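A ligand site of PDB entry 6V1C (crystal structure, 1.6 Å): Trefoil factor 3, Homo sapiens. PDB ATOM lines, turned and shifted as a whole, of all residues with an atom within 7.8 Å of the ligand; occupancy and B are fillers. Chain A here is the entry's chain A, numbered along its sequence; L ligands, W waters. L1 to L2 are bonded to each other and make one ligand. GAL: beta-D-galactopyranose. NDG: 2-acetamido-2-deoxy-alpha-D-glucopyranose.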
ATOM      1  N   ARG A  18      14.571  19.694 -22.226  1.00  0.00           N
ATOM      2  CA  ARG A  18      13.198  20.100 -22.464  1.00  0.00           C
ATOM      3  C   ARG A  18      12.875  20.070 -23.945  1.00  0.00           C
ATOM      4  O   ARG A  18      13.645  20.546 -24.773  1.00  0.00           O
ATOM      5  CB  ARG A  18      12.947  21.494 -21.927  1.00  0.00           C
ATOM      6  CG  ARG A  18      12.884  21.521 -20.418  1.00  0.00           C
ATOM      7  CD  ARG A  18      12.749  22.928 -19.912  1.00  0.00           C
ATOM      8  NE  ARG A  18      12.746  22.966 -18.465  1.00  0.00           N
ATOM      9  CZ  ARG A  18      12.529  24.064 -17.752  1.00  0.00           C
ATOM     10  NH1 ARG A  18      12.265  25.223 -18.342  1.00  0.00           N
ATOM     11  NH2 ARG A  18      12.569  23.992 -16.431  1.00  0.00           N
ATOM     12  N   VAL A  19      11.716  19.522 -24.260  1.00  0.00           N
ATOM     13  CA  VAL A  19      11.177  19.530 -25.611  1.00  0.00           C
ATOM     14  C   VAL A  19      10.059  20.572 -25.674  1.00  0.00           C
ATOM     15  O   VAL A  19       9.054  20.466 -24.964  1.00  0.00           O
ATOM     16  CB  VAL A  19      10.676  18.143 -26.002  1.00  0.00           C
ATOM     17  CG1 VAL A  19      10.145  18.182 -27.399  1.00  0.00           C
ATOM     18  CG2 VAL A  19      11.808  17.112 -25.860  1.00  0.00           C
ATOM     19  N   ASP A  20      10.244  21.585 -26.522  1.00  0.00           N
ATOM     20  CA  ASP A  20       9.281  22.666 -26.629  1.00  0.00           C
ATOM     21  C   ASP A  20       7.901  22.127 -27.014  1.00  0.00           C
ATOM     22  O   ASP A  20       7.750  21.351 -27.975  1.00  0.00           O
ATOM     23  CB  ASP A  20       9.784  23.698 -27.635  1.00  0.00           C
ATOM     24  CG  ASP A  20       9.064  25.015 -27.570  1.00  0.00           C
ATOM     25  OD1 ASP A  20       8.187  25.193 -26.700  1.00  0.00           O
ATOM     26  OD2 ASP A  20       9.400  25.890 -28.413  1.00  0.00           O
ATOM     27  N   CYS A  21       6.902  22.524 -26.240  1.00  0.00           N
ATOM     28  CA  CYS A  21       5.512  22.208 -26.463  1.00  0.00           C
ATOM     29  C   CYS A  21       4.711  23.440 -26.877  1.00  0.00           C
ATOM     30  O   CYS A  21       3.521  23.328 -27.194  1.00  0.00           O
ATOM     31  CB  CYS A  21       4.918  21.607 -25.194  1.00  0.00           C
ATOM     32  SG  CYS A  21       3.160  21.297 -25.174  1.00  0.00           S
ATOM     33  N   GLY A  22       5.340  24.597 -26.862  1.00  0.00           N
ATOM     34  CA  GLY A  22       4.662  25.812 -27.236  1.00  0.00           C
ATOM     35  C   GLY A  22       5.414  26.594 -28.293  1.00  0.00           C
ATOM     36  O   GLY A  22       5.841  26.052 -29.320  1.00  0.00           O
ATOM     37  N   TYR A  23       5.578  27.883 -28.011  1.00  0.00           N
ATOM     38  CA  TYR A  23       6.088  28.885 -28.945  1.00  0.00           C
ATOM     39  C   TYR A  23       6.341  30.146 -28.141  1.00  0.00           C
ATOM     40  O   TYR A  23       5.798  30.289 -27.044  1.00  0.00           O
ATOM     41  CB  TYR A  23       5.082  29.147 -30.092  1.00  0.00           C
ATOM     42  CG  TYR A  23       3.677  29.325 -29.571  1.00  0.00           C
ATOM     43  CD1 TYR A  23       3.218  30.563 -29.160  1.00  0.00           C
ATOM     44  CD2 TYR A  23       2.826  28.242 -29.446  1.00  0.00           C
ATOM     45  CE1 TYR A  23       1.937  30.712 -28.652  1.00  0.00           C
ATOM     46  CE2 TYR A  23       1.570  28.378 -28.925  1.00  0.00           C
ATOM     47  CZ  TYR A  23       1.126  29.610 -28.533  1.00  0.00           C
ATOM     48  OH  TYR A  23      -0.149  29.704 -28.010  1.00  0.00           O
ATOM     49  N   PRO A  24       7.157  31.061 -28.657  1.00  0.00           N
ATOM     50  CA  PRO A  24       7.393  32.310 -27.919  1.00  0.00           C
ATOM     51  C   PRO A  24       6.089  33.004 -27.527  1.00  0.00           C
ATOM     52  O   PRO A  24       5.171  33.147 -28.333  1.00  0.00           O
ATOM     53  CB  PRO A  24       8.211  33.136 -28.912  1.00  0.00           C
ATOM     54  CG  PRO A  24       8.930  32.050 -29.729  1.00  0.00           C
ATOM     55  CD  PRO A  24       7.907  31.012 -29.915  1.00  0.00           C
ATOM     56  N   HIS A  25       6.031  33.426 -26.270  1.00  0.00           N
ATOM     57  CA  HIS A  25       4.901  34.150 -25.680  1.00  0.00           C
ATOM     58  C   HIS A  25       3.669  33.295 -25.494  1.00  0.00           C
ATOM     59  O   HIS A  25       2.574  33.820 -25.263  1.00  0.00           O
ATOM     60  CB  HIS A  25       4.554  35.390 -26.498  1.00  0.00           C
ATOM     61  CG  HIS A  25       5.752  36.230 -26.802  1.00  0.00           C
ATOM     62  ND1 HIS A  25       6.357  37.037 -25.867  1.00  0.00           N
ATOM     63  CD2 HIS A  25       6.483  36.354 -27.940  1.00  0.00           C
ATOM     64  CE1 HIS A  25       7.401  37.621 -26.416  1.00  0.00           C
ATOM     65  NE2 HIS A  25       7.496  37.224 -27.673  1.00  0.00           N
ATOM     66  N   VAL A  26       3.825  31.971 -25.538  1.00  0.00           N
ATOM     67  CA  VAL A  26       2.737  31.092 -25.156  1.00  0.00           C
ATOM     68  C   VAL A  26       2.344  31.396 -23.712  1.00  0.00           C
ATOM     69  O   VAL A  26       3.201  31.614 -22.848  1.00  0.00           O
ATOM     70  CB  VAL A  26       3.136  29.614 -25.358  1.00  0.00           C
ATOM     71  CG1 VAL A  26       4.316  29.238 -24.477  1.00  0.00           C
ATOM     72  CG2 VAL A  26       1.939  28.673 -25.093  1.00  0.00           C
ATOM     73  N   THR A  27       1.061  31.377 -23.442  1.00  0.00           N
ATOM     74  CA  THR A  27       0.623  31.629 -22.065  1.00  0.00           C
ATOM     75  C   THR A  27       0.638  30.361 -21.245  1.00  0.00           C
ATOM     76  O   THR A  27       0.503  29.259 -21.779  1.00  0.00           O
ATOM     77  CB  THR A  27      -0.789  32.202 -22.031  1.00  0.00           C
ATOM     78  OG1 THR A  27      -1.686  31.215 -22.545  1.00  0.00           O
ATOM     79  CG2 THR A  27      -0.925  33.456 -22.844  1.00  0.00           C
ATOM     80  N   CYS A  31      -0.345  26.523 -22.358  1.00  0.00           N
ATOM     81  CA  CYS A  31       0.568  25.432 -22.067  1.00  0.00           C
ATOM     82  C   CYS A  31      -0.149  24.334 -21.299  1.00  0.00           C
ATOM     83  O   CYS A  31      -0.079  23.149 -21.674  1.00  0.00           O
ATOM     84  CB  CYS A  31       1.776  25.966 -21.269  1.00  0.00           C
ATOM     85  SG  CYS A  31       3.119  24.763 -21.176  1.00  0.00           S
ATOM     86  N   CYS A  37       4.072  21.326 -19.389  1.00  0.00           N
ATOM     87  CA  CYS A  37       4.657  21.929 -18.204  1.00  0.00           C
ATOM     88  C   CYS A  37       5.101  23.352 -18.496  1.00  0.00           C
ATOM     89  O   CYS A  37       5.735  23.606 -19.529  1.00  0.00           O
ATOM     90  CB  CYS A  37       5.878  21.134 -17.749  1.00  0.00           C
ATOM     91  SG  CYS A  37       5.589  19.389 -17.444  1.00  0.00           S
ATOM     92  N   PHE A  38       4.832  24.264 -17.561  1.00  0.00           N
ATOM     93  CA  PHE A  38       5.259  25.647 -17.694  1.00  0.00           C
ATOM     94  C   PHE A  38       6.271  25.974 -16.616  1.00  0.00           C
ATOM     95  O   PHE A  38       6.086  25.622 -15.446  1.00  0.00           O
ATOM     96  CB  PHE A  38       4.088  26.615 -17.649  1.00  0.00           C
ATOM     97  CG  PHE A  38       4.456  27.997 -18.083  1.00  0.00           C
ATOM     98  CD1 PHE A  38       4.356  28.374 -19.392  1.00  0.00           C
ATOM     99  CD2 PHE A  38       4.970  28.895 -17.174  1.00  0.00           C
ATOM    100  CE1 PHE A  38       4.737  29.646 -19.796  1.00  0.00           C
ATOM    101  CE2 PHE A  38       5.366  30.187 -17.578  1.00  0.00           C
ATOM    102  CZ  PHE A  38       5.230  30.559 -18.876  1.00  0.00           C
ATOM    103  N   ASP A  39       7.359  26.622 -17.008  1.00  0.00           N
ATOM    104  CA  ASP A  39       8.369  27.087 -16.064  1.00  0.00           C
ATOM    105  C   ASP A  39       9.096  28.257 -16.697  1.00  0.00           C
ATOM    106  O   ASP A  39       9.738  28.104 -17.737  1.00  0.00           O
ATOM    107  CB  ASP A  39       9.356  25.967 -15.718  1.00  0.00           C
ATOM    108  CG  ASP A  39      10.401  26.356 -14.680  1.00  0.00           C
ATOM    109  OD1 ASP A  39      10.203  27.334 -13.930  1.00  0.00           O
ATOM    110  OD2 ASP A  39      11.450  25.666 -14.616  1.00  0.00           O
ATOM    111  N   SER A  40       8.975  29.437 -16.091  1.00  0.00           N
ATOM    112  CA  SER A  40       9.662  30.635 -16.552  1.00  0.00           C
ATOM    113  C   SER A  40      10.890  30.984 -15.721  1.00  0.00           C
ATOM    114  O   SER A  40      11.460  32.054 -15.909  1.00  0.00           O
ATOM    115  CB  SER A  40       8.689  31.798 -16.558  1.00  0.00           C
ATOM    116  OG  SER A  40       8.193  32.042 -15.244  1.00  0.00           O
ATOM    117  N   ILE A  42      13.908  29.702 -15.582  1.00  0.00           N
ATOM    118  CA  ILE A  42      15.176  29.629 -16.304  1.00  0.00           C
ATOM    119  C   ILE A  42      15.011  30.354 -17.633  1.00  0.00           C
ATOM    120  O   ILE A  42      14.198  29.913 -18.470  1.00  0.00           O
ATOM    121  CB  ILE A  42      15.650  28.188 -16.522  1.00  0.00           C
ATOM    122  CG1 ILE A  42      15.670  27.412 -15.199  1.00  0.00           C
ATOM    123  CG2 ILE A  42      17.020  28.182 -17.143  1.00  0.00           C
ATOM    124  CD1 ILE A  42      15.811  25.923 -15.388  1.00  0.00           C
ATOM    125  N   PRO A  43      15.736  31.418 -17.896  1.00  0.00           N
ATOM    126  CA  PRO A  43      15.613  32.073 -19.195  1.00  0.00           C
ATOM    127  C   PRO A  43      16.369  31.314 -20.275  1.00  0.00           C
ATOM    128  O   PRO A  43      17.298  30.554 -20.004  1.00  0.00           O
ATOM    129  CB  PRO A  43      16.233  33.446 -18.951  1.00  0.00           C
ATOM    130  CG  PRO A  43      17.221  33.202 -17.881  1.00  0.00           C
ATOM    131  CD  PRO A  43      16.638  32.153 -16.984  1.00  0.00           C
ATOM    132  N   GLY A  44      15.919  31.505 -21.510  1.00  0.00           N
ATOM    133  CA  GLY A  44      16.666  31.039 -22.661  1.00  0.00           C
ATOM    134  C   GLY A  44      16.513  29.582 -22.984  1.00  0.00           C
ATOM    135  O   GLY A  44      17.318  29.032 -23.736  1.00  0.00           O
ATOM    136  N   VAL A  45      15.479  28.945 -22.433  1.00  0.00           N
ATOM    137  CA  VAL A  45      15.143  27.538 -22.666  1.00  0.00           C
ATOM    138  C   VAL A  45      13.623  27.470 -22.773  1.00  0.00           C
ATOM    139  O   VAL A  45      12.937  28.429 -22.379  1.00  0.00           O
ATOM    140  CB  VAL A  45      15.648  26.625 -21.530  1.00  0.00           C
ATOM    141  CG1 VAL A  45      17.127  26.837 -21.321  1.00  0.00           C
ATOM    142  CG2 VAL A  45      14.880  26.883 -20.211  1.00  0.00           C
ATOM    143  N   PRO A  46      13.059  26.370 -23.275  1.00  0.00           N
ATOM    144  CA  PRO A  46      11.597  26.287 -23.413  1.00  0.00           C
ATOM    145  C   PRO A  46      10.932  26.511 -22.070  1.00  0.00           C
ATOM    146  O   PRO A  46      11.249  25.869 -21.063  1.00  0.00           O
ATOM    147  CB  PRO A  46      11.373  24.852 -23.932  1.00  0.00           C
ATOM    148  CG  PRO A  46      12.602  24.535 -24.648  1.00  0.00           C
ATOM    149  CD  PRO A  46      13.699  25.154 -23.802  1.00  0.00           C
ATOM    150  N   TRP A  47       9.983  27.435 -22.065  1.00  0.00           N
ATOM    151  CA  TRP A  47       9.176  27.671 -20.895  1.00  0.00           C
ATOM    152  C   TRP A  47       7.937  26.792 -20.864  1.00  0.00           C
ATOM    153  O   TRP A  47       7.321  26.656 -19.813  1.00  0.00           O
ATOM    154  CB  TRP A  47       8.769  29.136 -20.833  1.00  0.00           C
ATOM    155  CG  TRP A  47       9.829  30.050 -20.358  1.00  0.00           C
ATOM    156  CD1 TRP A  47      11.133  29.749 -20.056  1.00  0.00           C
ATOM    157  CD2 TRP A  47       9.664  31.434 -20.075  1.00  0.00           C
ATOM    158  NE1 TRP A  47      11.789  30.863 -19.614  1.00  0.00           N
ATOM    159  CE2 TRP A  47      10.911  31.913 -19.627  1.00  0.00           C
ATOM    160  CE3 TRP A  47       8.592  32.332 -20.178  1.00  0.00           C
ATOM    161  CZ2 TRP A  47      11.113  33.244 -19.259  1.00  0.00           C
ATOM    162  CZ3 TRP A  47       8.796  33.646 -19.834  1.00  0.00           C
ATOM    163  CH2 TRP A  47      10.032  34.093 -19.365  1.00  0.00           C
ATOM    164  N   CYS A  48       7.571  26.197 -21.991  1.00  0.00           N
ATOM    165  CA  CYS A  48       6.435  25.295 -22.090  1.00  0.00           C
ATOM    166  C   CYS A  48       6.947  24.025 -22.730  1.00  0.00           C
ATOM    167  O   CYS A  48       7.354  24.056 -23.905  1.00  0.00           O
ATOM    168  CB  CYS A  48       5.317  25.913 -22.911  1.00  0.00           C
ATOM    169  SG  CYS A  48       3.909  24.815 -23.116  1.00  0.00           S
ATOM    170  N   PHE A  49       6.960  22.925 -21.980  1.00  0.00           N
ATOM    171  CA  PHE A  49       7.675  21.744 -22.449  1.00  0.00           C
ATOM    172  C   PHE A  49       6.927  20.456 -22.141  1.00  0.00           C
ATOM    173  O   PHE A  49       6.070  20.418 -21.264  1.00  0.00           O
ATOM    174  CB  PHE A  49       9.107  21.692 -21.850  1.00  0.00           C
ATOM    175  CG  PHE A  49       9.153  21.831 -20.357  1.00  0.00           C
ATOM    176  CD1 PHE A  49       9.188  23.074 -19.776  1.00  0.00           C
ATOM    177  CD2 PHE A  49       9.173  20.700 -19.535  1.00  0.00           C
ATOM    178  CE1 PHE A  49       9.244  23.202 -18.409  1.00  0.00           C
ATOM    179  CE2 PHE A  49       9.216  20.827 -18.156  1.00  0.00           C
ATOM    180  CZ  PHE A  49       9.252  22.065 -17.584  1.00  0.00           C
HETATM  181  C1  GAL L   1      10.576  34.816 -24.093  1.00  0.00           C
HETATM  182  C2  GAL L   1       9.439  34.043 -24.738  1.00  0.00           C
HETATM  183  C3  GAL L   1       9.036  32.889 -23.843  1.00  0.00           C
HETATM  184  C4  GAL L   1      10.267  32.032 -23.552  1.00  0.00           C
HETATM  185  C5  GAL L   1      11.386  32.888 -22.980  1.00  0.00           C
HETATM  186  C6  GAL L   1      12.674  32.156 -22.734  1.00  0.00           C
HETATM  187  O1  GAL L   1      10.930  35.828 -24.945  1.00  0.00           O
HETATM  188  O2  GAL L   1       8.332  34.901 -24.977  1.00  0.00           O
HETATM  189  O3  GAL L   1       7.991  32.141 -24.457  1.00  0.00           O
HETATM  190  O4  GAL L   1      10.719  31.352 -24.737  1.00  0.00           O
HETATM  191  O5  GAL L   1      11.684  33.952 -23.899  1.00  0.00           O
HETATM  192  O6  GAL L   1      13.609  33.004 -22.068  1.00  0.00           O
HETATM  193  C1  NDG L   2      11.085  29.996 -24.561  1.00  0.00           C
HETATM  194  C2  NDG L   2      11.891  29.489 -25.762  1.00  0.00           C
HETATM  195  C3  NDG L   2      11.010  29.436 -27.016  1.00  0.00           C
HETATM  196  C4  NDG L   2       9.825  28.551 -26.716  1.00  0.00           C
HETATM  197  C5  NDG L   2       9.071  29.102 -25.514  1.00  0.00           C
HETATM  198  C6  NDG L   2       7.911  28.239 -25.091  1.00  0.00           C
HETATM  199  C7  NDG L   2      14.309  29.787 -25.986  1.00  0.00           C
HETATM  200  C8  NDG L   2      15.428  30.754 -26.180  1.00  0.00           C
HETATM  201  O5  NDG L   2       9.944  29.186 -24.370  1.00  0.00           O
HETATM  202  O3  NDG L   2      11.764  28.915 -28.115  1.00  0.00           O
HETATM  203  O4  NDG L   2       8.951  28.498 -27.833  1.00  0.00           O
HETATM  204  O6  NDG L   2       8.350  26.975 -24.602  1.00  0.00           O
HETATM  205  O7  NDG L   2      14.507  28.587 -25.818  1.00  0.00           O
HETATM  206  N2  NDG L   2      13.076  30.302 -26.000  1.00  0.00           N
HETATM  207  O   HOH W   1      10.467  28.063 -30.739  1.00  0.00           O
HETATM  208  O   HOH W   2       5.942  32.146 -22.728  1.00  0.00           O
HETATM  209  O   HOH W   3      13.200  33.147 -26.189  1.00  0.00           O
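N of Cys 48 is in hydrogen-bond range of O6 of NDG L2, 2.8 Å away. ND1 of His 25 sits at hydrogen-bond distance from O2 of GAL L1 (3.0 Å). The backbone NH of Gly 44 sits at hydrogen-bond distance from an oxygen (O6) of GAL L1 (2.8 Å). The side-chain carboxylate (OD2) of Asp 20 is in hydrogen-bond range of an oxygen (O4) of NDG L2 (2.7 Å). N of Trp 47 lies within hydrogen-bond range of O5 of NDG L2, 2.9 Å away. The backbone NH of Tyr 23 sits close to an oxygen (O4) of NDG L2 (3.4 Å). O3 of GAL L1 lies within hydrogen-bond range of N of His 25 (3.0 Å). The backbone carbonyl oxygen (O) of Cys 48 is in hydrogen-bond range of an oxygen (O6) of NDG L2 (3.2 Å).
The backbone NH (N) of Asp 39 is in hydrogen-bond range of the backbone carbonyl oxygen (O) of Trp 47 (2.8 Å). O of Pro 46 lies within hydrogen-bond range of NH1 of Arg 18 (3.0 Å). The side-chain sulfur (SG) of Cys 48 forms a disulfide with the side-chain sulfur (SG) of Cys 31 (2.1 Å). The backbone NH of Cys 21 lies within hydrogen-bond range of the backbone carbonyl oxygen of Cys 48 (2.8 Å). The indole nitrogen of Trp 47 sits at hydrogen-bond distance from the backbone carbonyl oxygen of Ile 42 (2.8 Å). The backbone NH of Gly 22 is in hydrogen-bond range of the side-chain carboxylate of Asp 20 (2.9 Å).
N of Pro 24 sits close to O4 of NDG L2, 3.2 Å away. Merely in contact with the ligand: Val 26 (3.8 Å), Pro 43 (3.6 Å), Val 45 (3.3 Å) and Pro 46 (3.5 Å). Hydrophobic or aromatic side chains within 4 Å of the ligand: Pro 24, His 25, Val 26, Pro 46 and Trp 47. Of the 23 residues printed, 11 come within 4 Å of the ligand.
Water W2 bridges an oxygen (O3) of GAL L1 and the backbone carbonyl oxygen of Val 26. Water W1 bridges O3 of NDG L2 (3.0 Å) and OD2 of Asp 20 (3.4 Å).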
